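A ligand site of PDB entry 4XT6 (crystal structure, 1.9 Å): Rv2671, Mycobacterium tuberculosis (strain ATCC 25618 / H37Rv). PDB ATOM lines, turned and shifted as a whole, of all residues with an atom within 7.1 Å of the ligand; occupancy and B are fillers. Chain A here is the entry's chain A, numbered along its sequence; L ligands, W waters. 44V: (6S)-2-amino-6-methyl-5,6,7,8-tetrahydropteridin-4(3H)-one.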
ATOM      1  N   ALA A  43      22.702  38.034  32.041  1.00  0.00           N
ATOM      2  CA  ALA A  43      22.318  37.030  31.062  1.00  0.00           C
ATOM      3  C   ALA A  43      21.409  36.047  31.769  1.00  0.00           C
ATOM      4  O   ALA A  43      21.589  35.796  32.959  1.00  0.00           O
ATOM      5  CB  ALA A  43      23.550  36.290  30.525  1.00  0.00           C
ATOM      6  N   ASN A  44      20.440  35.498  31.033  1.00  0.00           N
ATOM      7  CA  ASN A  44      19.609  34.418  31.554  1.00  0.00           C
ATOM      8  C   ASN A  44      19.586  33.275  30.562  1.00  0.00           C
ATOM      9  O   ASN A  44      19.160  33.461  29.413  1.00  0.00           O
ATOM     10  CB  ASN A  44      18.196  34.892  31.855  1.00  0.00           C
ATOM     11  CG  ASN A  44      17.348  33.804  32.499  1.00  0.00           C
ATOM     12  OD1 ASN A  44      17.862  32.932  33.187  1.00  0.00           O
ATOM     13  ND2 ASN A  44      16.022  33.854  32.269  1.00  0.00           N
ATOM     14  N   PHE A  45      20.066  32.111  30.982  1.00  0.00           N
ATOM     15  CA  PHE A  45      20.127  30.945  30.106  1.00  0.00           C
ATOM     16  C   PHE A  45      19.703  29.699  30.845  1.00  0.00           C
ATOM     17  O   PHE A  45      19.613  29.702  32.077  1.00  0.00           O
ATOM     18  CB  PHE A  45      21.550  30.765  29.576  1.00  0.00           C
ATOM     19  CG  PHE A  45      21.884  31.727  28.486  1.00  0.00           C
ATOM     20  CD1 PHE A  45      22.131  33.067  28.780  1.00  0.00           C
ATOM     21  CD2 PHE A  45      21.889  31.324  27.172  1.00  0.00           C
ATOM     22  CE1 PHE A  45      22.399  33.979  27.769  1.00  0.00           C
ATOM     23  CE2 PHE A  45      22.167  32.214  26.156  1.00  0.00           C
ATOM     24  CZ  PHE A  45      22.412  33.555  26.459  1.00  0.00           C
ATOM     25  N   ILE A  46      19.462  28.617  30.092  1.00  0.00           N
ATOM     26  CA  ILE A  46      19.144  27.343  30.721  1.00  0.00           C
ATOM     27  C   ILE A  46      20.019  26.290  30.065  1.00  0.00           C
ATOM     28  O   ILE A  46      20.332  26.369  28.880  1.00  0.00           O
ATOM     29  CB  ILE A  46      17.634  27.025  30.542  1.00  0.00           C
ATOM     30  CG1 ILE A  46      17.267  25.675  31.163  1.00  0.00           C
ATOM     31  CG2 ILE A  46      17.246  27.066  29.070  1.00  0.00           C
ATOM     32  CD1 ILE A  46      15.744  25.434  31.204  1.00  0.00           C
ATOM     33  N   SER A  47      20.451  25.301  30.833  1.00  0.00           N
ATOM     34  CA  SER A  47      21.220  24.235  30.228  1.00  0.00           C
ATOM     35  C   SER A  47      20.989  22.935  30.964  1.00  0.00           C
ATOM     36  O   SER A  47      20.444  22.919  32.064  1.00  0.00           O
ATOM     37  CB  SER A  47      22.705  24.565  30.228  1.00  0.00           C
ATOM     38  OG  SER A  47      23.192  24.625  31.552  1.00  0.00           O
ATOM     39  N   ALA A  53      22.480  23.273  25.652  1.00  0.00           N
ATOM     40  CA  ALA A  53      21.591  24.430  25.709  1.00  0.00           C
ATOM     41  C   ALA A  53      20.297  24.204  24.957  1.00  0.00           C
ATOM     42  O   ALA A  53      19.335  24.953  25.148  1.00  0.00           O
ATOM     43  CB  ALA A  53      22.276  25.653  25.134  1.00  0.00           C
ATOM     44  N   THR A  58      15.820  24.582  20.226  1.00  0.00           N
ATOM     45  CA  THR A  58      15.401  25.456  21.320  1.00  0.00           C
ATOM     46  C   THR A  58      15.618  24.815  22.690  1.00  0.00           C
ATOM     47  O   THR A  58      15.899  23.623  22.791  1.00  0.00           O
ATOM     48  CB  THR A  58      13.916  25.853  21.202  1.00  0.00           C
ATOM     49  OG1 THR A  58      13.130  24.701  20.876  1.00  0.00           O
ATOM     50  CG2 THR A  58      13.734  26.901  20.109  1.00  0.00           C
ATOM     51  N   SER A  59      15.476  25.627  23.734  1.00  0.00           N
ATOM     52  CA  SER A  59      15.723  25.171  25.095  1.00  0.00           C
ATOM     53  C   SER A  59      14.419  24.886  25.851  1.00  0.00           C
ATOM     54  O   SER A  59      14.446  24.317  26.959  1.00  0.00           O
ATOM     55  CB  SER A  59      16.515  26.246  25.834  1.00  0.00           C
ATOM     56  OG  SER A  59      15.960  27.530  25.609  1.00  0.00           O
ATOM     57  N   GLY A  60      13.294  25.280  25.251  1.00  0.00           N
ATOM     58  CA  GLY A  60      11.977  25.175  25.857  1.00  0.00           C
ATOM     59  C   GLY A  60      11.592  23.825  26.418  1.00  0.00           C
ATOM     60  O   GLY A  60      10.935  23.739  27.468  1.00  0.00           O
ATOM     61  N   ALA A  61      11.990  22.751  25.741  1.00  0.00           N
ATOM     62  CA  ALA A  61      11.712  21.394  26.202  1.00  0.00           C
ATOM     63  C   ALA A  61      12.231  21.137  27.613  1.00  0.00           C
ATOM     64  O   ALA A  61      11.672  20.319  28.347  1.00  0.00           O
ATOM     65  CB  ALA A  61      12.317  20.395  25.237  1.00  0.00           C
ATOM     66  N   MET A  62      13.306  21.820  27.989  1.00  0.00           N
ATOM     67  CA  MET A  62      13.880  21.622  29.328  1.00  0.00           C
ATOM     68  C   MET A  62      13.273  22.571  30.360  1.00  0.00           C
ATOM     69  O   MET A  62      13.507  22.430  31.557  1.00  0.00           O
ATOM     70  CB  MET A  62      15.397  21.842  29.286  1.00  0.00           C
ATOM     71  CG  MET A  62      16.154  20.839  28.447  1.00  0.00           C
ATOM     72  SD  MET A  62      17.945  21.025  28.650  1.00  0.00           S
ATOM     73  CE  MET A  62      18.197  22.633  27.921  1.00  0.00           C
ATOM     74  N   ALA A  63      12.488  23.535  29.900  1.00  0.00           N
ATOM     75  CA  ALA A  63      11.973  24.578  30.785  1.00  0.00           C
ATOM     76  C   ALA A  63      10.583  24.261  31.314  1.00  0.00           C
ATOM     77  O   ALA A  63       9.624  24.193  30.541  1.00  0.00           O
ATOM     78  CB  ALA A  63      11.945  25.917  30.074  1.00  0.00           C
ATOM     79  N   ASP A  67      10.977  27.654  35.792  1.00  0.00           N
ATOM     80  CA  ASP A  67      11.895  28.406  34.942  1.00  0.00           C
ATOM     81  C   ASP A  67      11.159  29.464  34.170  1.00  0.00           C
ATOM     82  O   ASP A  67      11.679  30.560  33.977  1.00  0.00           O
ATOM     83  CB  ASP A  67      12.672  27.498  33.994  1.00  0.00           C
ATOM     84  CG  ASP A  67      13.592  28.285  33.077  1.00  0.00           C
ATOM     85  OD1 ASP A  67      14.593  28.850  33.579  1.00  0.00           O
ATOM     86  OD2 ASP A  67      13.318  28.357  31.864  1.00  0.00           O
ATOM     87  N   ARG A  68       9.936  29.164  33.725  1.00  0.00           N
ATOM     88  CA  ARG A  68       9.136  30.193  33.041  1.00  0.00           C
ATOM     89  C   ARG A  68       8.870  31.363  33.975  1.00  0.00           C
ATOM     90  O   ARG A  68       8.880  32.540  33.559  1.00  0.00           O
ATOM     91  CB  ARG A  68       7.808  29.593  32.571  1.00  0.00           C
ATOM     92  CG  ARG A  68       7.960  28.620  31.429  1.00  0.00           C
ATOM     93  CD  ARG A  68       6.597  28.076  31.026  1.00  0.00           C
ATOM     94  NE  ARG A  68       6.657  27.387  29.739  1.00  0.00           N
ATOM     95  CZ  ARG A  68       5.782  27.562  28.758  1.00  0.00           C
ATOM     96  NH1 ARG A  68       4.765  28.389  28.912  1.00  0.00           N
ATOM     97  NH2 ARG A  68       5.915  26.889  27.632  1.00  0.00           N
ATOM     98  N   VAL A  70      10.757  32.407  36.603  1.00  0.00           N
ATOM     99  CA  VAL A  70      11.972  33.219  36.695  1.00  0.00           C
ATOM    100  C   VAL A  70      12.256  34.034  35.413  1.00  0.00           C
ATOM    101  O   VAL A  70      12.590  35.214  35.466  1.00  0.00           O
ATOM    102  CB  VAL A  70      13.184  32.347  37.078  1.00  0.00           C
ATOM    103  CG1 VAL A  70      14.454  33.196  37.153  1.00  0.00           C
ATOM    104  CG2 VAL A  70      12.939  31.713  38.419  1.00  0.00           C
ATOM    105  N   PHE A  71      12.104  33.378  34.263  1.00  0.00           N
ATOM    106  CA  PHE A  71      12.341  33.988  32.954  1.00  0.00           C
ATOM    107  C   PHE A  71      11.494  35.264  32.801  1.00  0.00           C
ATOM    108  O   PHE A  71      11.980  36.366  32.437  1.00  0.00           O
ATOM    109  CB  PHE A  71      12.001  32.934  31.899  1.00  0.00           C
ATOM    110  CG  PHE A  71      12.269  33.354  30.482  1.00  0.00           C
ATOM    111  CD1 PHE A  71      13.516  33.130  29.908  1.00  0.00           C
ATOM    112  CD2 PHE A  71      11.280  33.950  29.726  1.00  0.00           C
ATOM    113  CE1 PHE A  71      13.761  33.511  28.594  1.00  0.00           C
ATOM    114  CE2 PHE A  71      11.518  34.337  28.409  1.00  0.00           C
ATOM    115  CZ  PHE A  71      12.759  34.115  27.854  1.00  0.00           C
ATOM    116  N   LEU A  74      12.625  38.104  35.167  1.00  0.00           N
ATOM    117  CA  LEU A  74      13.824  38.805  34.704  1.00  0.00           C
ATOM    118  C   LEU A  74      13.466  39.745  33.563  1.00  0.00           C
ATOM    119  O   LEU A  74      14.022  40.847  33.466  1.00  0.00           O
ATOM    120  CB  LEU A  74      14.917  37.820  34.273  1.00  0.00           C
ATOM    121  CG  LEU A  74      15.399  36.931  35.429  1.00  0.00           C
ATOM    122  CD1 LEU A  74      16.576  36.059  35.005  1.00  0.00           C
ATOM    123  CD2 LEU A  74      15.749  37.767  36.627  1.00  0.00           C
ATOM    124  N   THR A  87      19.088  34.642  16.795  1.00  0.00           N
ATOM    125  CA  THR A  87      18.034  34.165  17.687  1.00  0.00           C
ATOM    126  C   THR A  87      16.667  34.793  17.415  1.00  0.00           C
ATOM    127  O   THR A  87      15.639  34.237  17.816  1.00  0.00           O
ATOM    128  CB  THR A  87      18.413  34.366  19.162  1.00  0.00           C
ATOM    129  OG1 THR A  87      19.776  33.969  19.334  1.00  0.00           O
ATOM    130  CG2 THR A  87      17.559  33.511  20.076  1.00  0.00           C
ATOM    131  N   THR A 192      20.177  39.882  28.612  1.00  0.00           N
ATOM    132  CA  THR A 192      20.331  39.192  27.336  1.00  0.00           C
ATOM    133  C   THR A 192      19.946  37.733  27.474  1.00  0.00           C
ATOM    134  O   THR A 192      20.250  37.109  28.479  1.00  0.00           O
ATOM    135  CB  THR A 192      21.759  39.347  26.741  1.00  0.00           C
ATOM    136  OG1 THR A 192      21.799  38.728  25.451  1.00  0.00           O
ATOM    137  CG2 THR A 192      22.794  38.700  27.645  1.00  0.00           C
ATOM    138  N   GLU A 193      19.213  37.216  26.485  1.00  0.00           N
ATOM    139  CA  GLU A 193      18.778  35.827  26.525  1.00  0.00           C
ATOM    140  C   GLU A 193      19.436  35.021  25.409  1.00  0.00           C
ATOM    141  O   GLU A 193      19.131  33.853  25.216  1.00  0.00           O
ATOM    142  CB  GLU A 193      17.247  35.738  26.410  1.00  0.00           C
ATOM    143  CG  GLU A 193      16.505  36.281  27.630  1.00  0.00           C
ATOM    144  CD  GLU A 193      15.083  36.659  27.324  1.00  0.00           C
ATOM    145  OE1 GLU A 193      14.722  36.749  26.121  1.00  0.00           O
ATOM    146  OE2 GLU A 193      14.310  36.856  28.283  1.00  0.00           O
ATOM    147  N   GLY A 194      20.359  35.653  24.690  1.00  0.00           N
ATOM    148  CA  GLY A 194      21.094  34.939  23.655  1.00  0.00           C
ATOM    149  C   GLY A 194      21.137  35.681  22.351  1.00  0.00           C
ATOM    150  O   GLY A 194      20.807  36.878  22.307  1.00  0.00           O
ATOM    151  N   GLY A 195      21.529  34.994  21.283  1.00  0.00           N
ATOM    152  CA  GLY A 195      21.918  33.585  21.369  1.00  0.00           C
ATOM    153  C   GLY A 195      23.341  33.297  21.826  1.00  0.00           C
ATOM    154  O   GLY A 195      24.014  34.159  22.398  1.00  0.00           O
ATOM    155  N   CYS A 212      22.452  34.473  35.243  1.00  0.00           N
ATOM    156  CA  CYS A 212      21.426  33.677  35.892  1.00  0.00           C
ATOM    157  C   CYS A 212      21.289  32.414  35.075  1.00  0.00           C
ATOM    158  O   CYS A 212      21.036  32.467  33.871  1.00  0.00           O
ATOM    159  CB  CYS A 212      20.109  34.421  35.911  1.00  0.00           C
ATOM    160  SG  CYS A 212      20.232  35.862  36.969  1.00  0.00           S
ATOM    161  N   LEU A 213      21.466  31.267  35.710  1.00  0.00           N
ATOM    162  CA  LEU A 213      21.474  30.064  34.915  1.00  0.00           C
ATOM    163  C   LEU A 213      20.568  29.051  35.552  1.00  0.00           C
ATOM    164  O   LEU A 213      20.729  28.712  36.734  1.00  0.00           O
ATOM    165  CB  LEU A 213      22.903  29.502  34.819  1.00  0.00           C
ATOM    166  CG  LEU A 213      23.041  28.108  34.204  1.00  0.00           C
ATOM    167  CD1 LEU A 213      22.820  28.124  32.686  1.00  0.00           C
ATOM    168  CD2 LEU A 213      24.406  27.496  34.548  1.00  0.00           C
ATOM    169  N   THR A 214      19.611  28.577  34.780  1.00  0.00           N
ATOM    170  CA  THR A 214      18.795  27.477  35.192  1.00  0.00           C
ATOM    171  C   THR A 214      19.469  26.198  34.757  1.00  0.00           C
ATOM    172  O   THR A 214      19.751  25.990  33.569  1.00  0.00           O
ATOM    173  CB  THR A 214      17.412  27.553  34.558  1.00  0.00           C
ATOM    174  OG1 THR A 214      16.750  28.738  35.029  1.00  0.00           O
ATOM    175  CG2 THR A 214      16.613  26.315  34.937  1.00  0.00           C
ATOM    176  N   ARG A 225      24.704  22.024  21.388  1.00  0.00           N
ATOM    177  CA  ARG A 225      25.715  23.048  21.612  1.00  0.00           C
ATOM    178  C   ARG A 225      25.630  23.547  23.049  1.00  0.00           C
ATOM    179  O   ARG A 225      24.654  23.292  23.732  1.00  0.00           O
ATOM    180  CB  ARG A 225      25.437  24.216  20.666  1.00  0.00           C
ATOM    181  CG  ARG A 225      23.999  24.762  20.813  1.00  0.00           C
ATOM    182  CD  ARG A 225      23.857  26.193  20.267  1.00  0.00           C
ATOM    183  NE  ARG A 225      22.494  26.720  20.399  1.00  0.00           N
ATOM    184  CZ  ARG A 225      22.058  27.404  21.464  1.00  0.00           C
ATOM    185  NH1 ARG A 225      22.883  27.631  22.483  1.00  0.00           N
ATOM    186  NH2 ARG A 225      20.806  27.869  21.503  1.00  0.00           N
ATOM    187  N   TYR A 252      18.002  27.180  40.119  1.00  0.00           N
ATOM    188  CA  TYR A 252      17.963  28.519  39.533  1.00  0.00           C
ATOM    189  C   TYR A 252      19.059  29.302  40.203  1.00  0.00           C
ATOM    190  O   TYR A 252      18.939  29.681  41.374  1.00  0.00           O
ATOM    191  CB  TYR A 252      16.586  29.157  39.766  1.00  0.00           C
ATOM    192  CG  TYR A 252      15.485  28.250  39.308  1.00  0.00           C
ATOM    193  CD1 TYR A 252      15.135  28.173  37.957  1.00  0.00           C
ATOM    194  CD2 TYR A 252      14.802  27.429  40.192  1.00  0.00           C
ATOM    195  CE1 TYR A 252      14.133  27.337  37.515  1.00  0.00           C
ATOM    196  CE2 TYR A 252      13.798  26.580  39.761  1.00  0.00           C
ATOM    197  CZ  TYR A 252      13.470  26.535  38.425  1.00  0.00           C
ATOM    198  OH  TYR A 252      12.473  25.693  37.995  1.00  0.00           O
HETATM  199  C13 44V L   1      16.204  30.979  24.124  1.00  0.00           C
HETATM  200  C01 44V L   1      17.240  31.747  25.984  1.00  0.00           C
HETATM  201  C02 44V L   1      16.662  30.748  25.596  1.00  0.00           C
HETATM  202  N03 44V L   1      15.473  30.338  26.447  1.00  0.00           N
HETATM  203  C04 44V L   1      15.605  30.314  27.830  1.00  0.00           C
HETATM  204  C05 44V L   1      16.747  31.154  28.414  1.00  0.00           C
HETATM  205  N06 44V L   1      17.538  31.854  27.484  1.00  0.00           N
HETATM  206  N07 44V L   1      16.953  31.195  29.826  1.00  0.00           N
HETATM  207  C08 44V L   1      16.071  30.421  30.712  1.00  0.00           C
HETATM  208  N09 44V L   1      14.958  29.606  30.145  1.00  0.00           N
HETATM  209  C10 44V L   1      14.730  29.557  28.737  1.00  0.00           C
HETATM  210  O11 44V L   1      13.816  28.883  28.298  1.00  0.00           O
HETATM  211  N12 44V L   1      16.264  30.446  32.121  1.00  0.00           N
HETATM  212  O   HOH W   1      14.794  31.904  34.252  1.00  0.00           O
HETATM  213  O   HOH W   2      11.359  29.408  29.949  1.00  0.00           O
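A nitrogen (N09) of the ligand is in hydrogen-bond range of the side-chain carboxylate (OD2) of Asp 67 (2.7 Å).
O of Glu 193 sits close to N06 of the ligand (3.4 Å).
OG of Ser 59 sits at hydrogen-bond distance from N03 of the ligand, at 3.0 Å.
A nitrogen (N06) of the ligand sits at hydrogen-bond distance from the backbone carbonyl oxygen (O) of Asn 44 (3.0 Å).
OD1 of Asn 44 lies within hydrogen-bond range of N12 of the ligand, at 3.1 Å.
A nitrogen (N07) of the ligand lies close to the backbone NH (N) of Phe 45 (3.4 Å).
The backbone carbonyl oxygen of Phe 45 sits at hydrogen-bond distance from a nitrogen (N12) of the ligand, 3.4 Å away.
A nitrogen (N12) of the ligand lies within hydrogen-bond range of the side-chain hydroxyl (OG1) of Thr 214, at 3.4 Å.
The side-chain carboxylate (OD1) of Asp 67 is in hydrogen-bond range of the side-chain hydroxyl (OG1) of Thr 214 (2.6 Å).
The side-chain hydroxyl (OH) of Tyr 252 is in hydrogen-bond range of the backbone NH (N) of Asp 67, at 3.3 Å.
OD1 of Asn 44 lies close to O of Cys 212 (3.3 Å).
The backbone NH of Asn 44 lies within hydrogen-bond range of the backbone carbonyl oxygen of Thr 192 (3.0 Å).
The backbone NH (N) of Thr 214 lies within hydrogen-bond range of the backbone carbonyl oxygen (O) of Phe 45 (2.9 Å).
The backbone NH (N) of Phe 45 sits at hydrogen-bond distance from the backbone carbonyl oxygen (O) of Cys 212, 3.1 Å away.
The backbone NH of Ser 47 sits at hydrogen-bond distance from the backbone carbonyl oxygen of Thr 214 (2.9 Å).
Ile 46 touches the ligand.
CB of Ala 63 touches O11 of the ligand (3.9 Å).
Phe 71 touches the ligand.
Hydrophobic or aromatic side chains within 4 Å of the ligand: Ile 46, Ala 63 and Phe 71.
Within 4 Å of the ligand: Asn 44, Phe 45, Ile 46, Ser 59, Ala 63, Asp 67, Phe 71, Glu 193 and Thr 214.
Water W2 bridges the side-chain carboxylate of Asp 67 (2.9 Å) and an oxygen (O11) of the ligand (3.0 Å).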
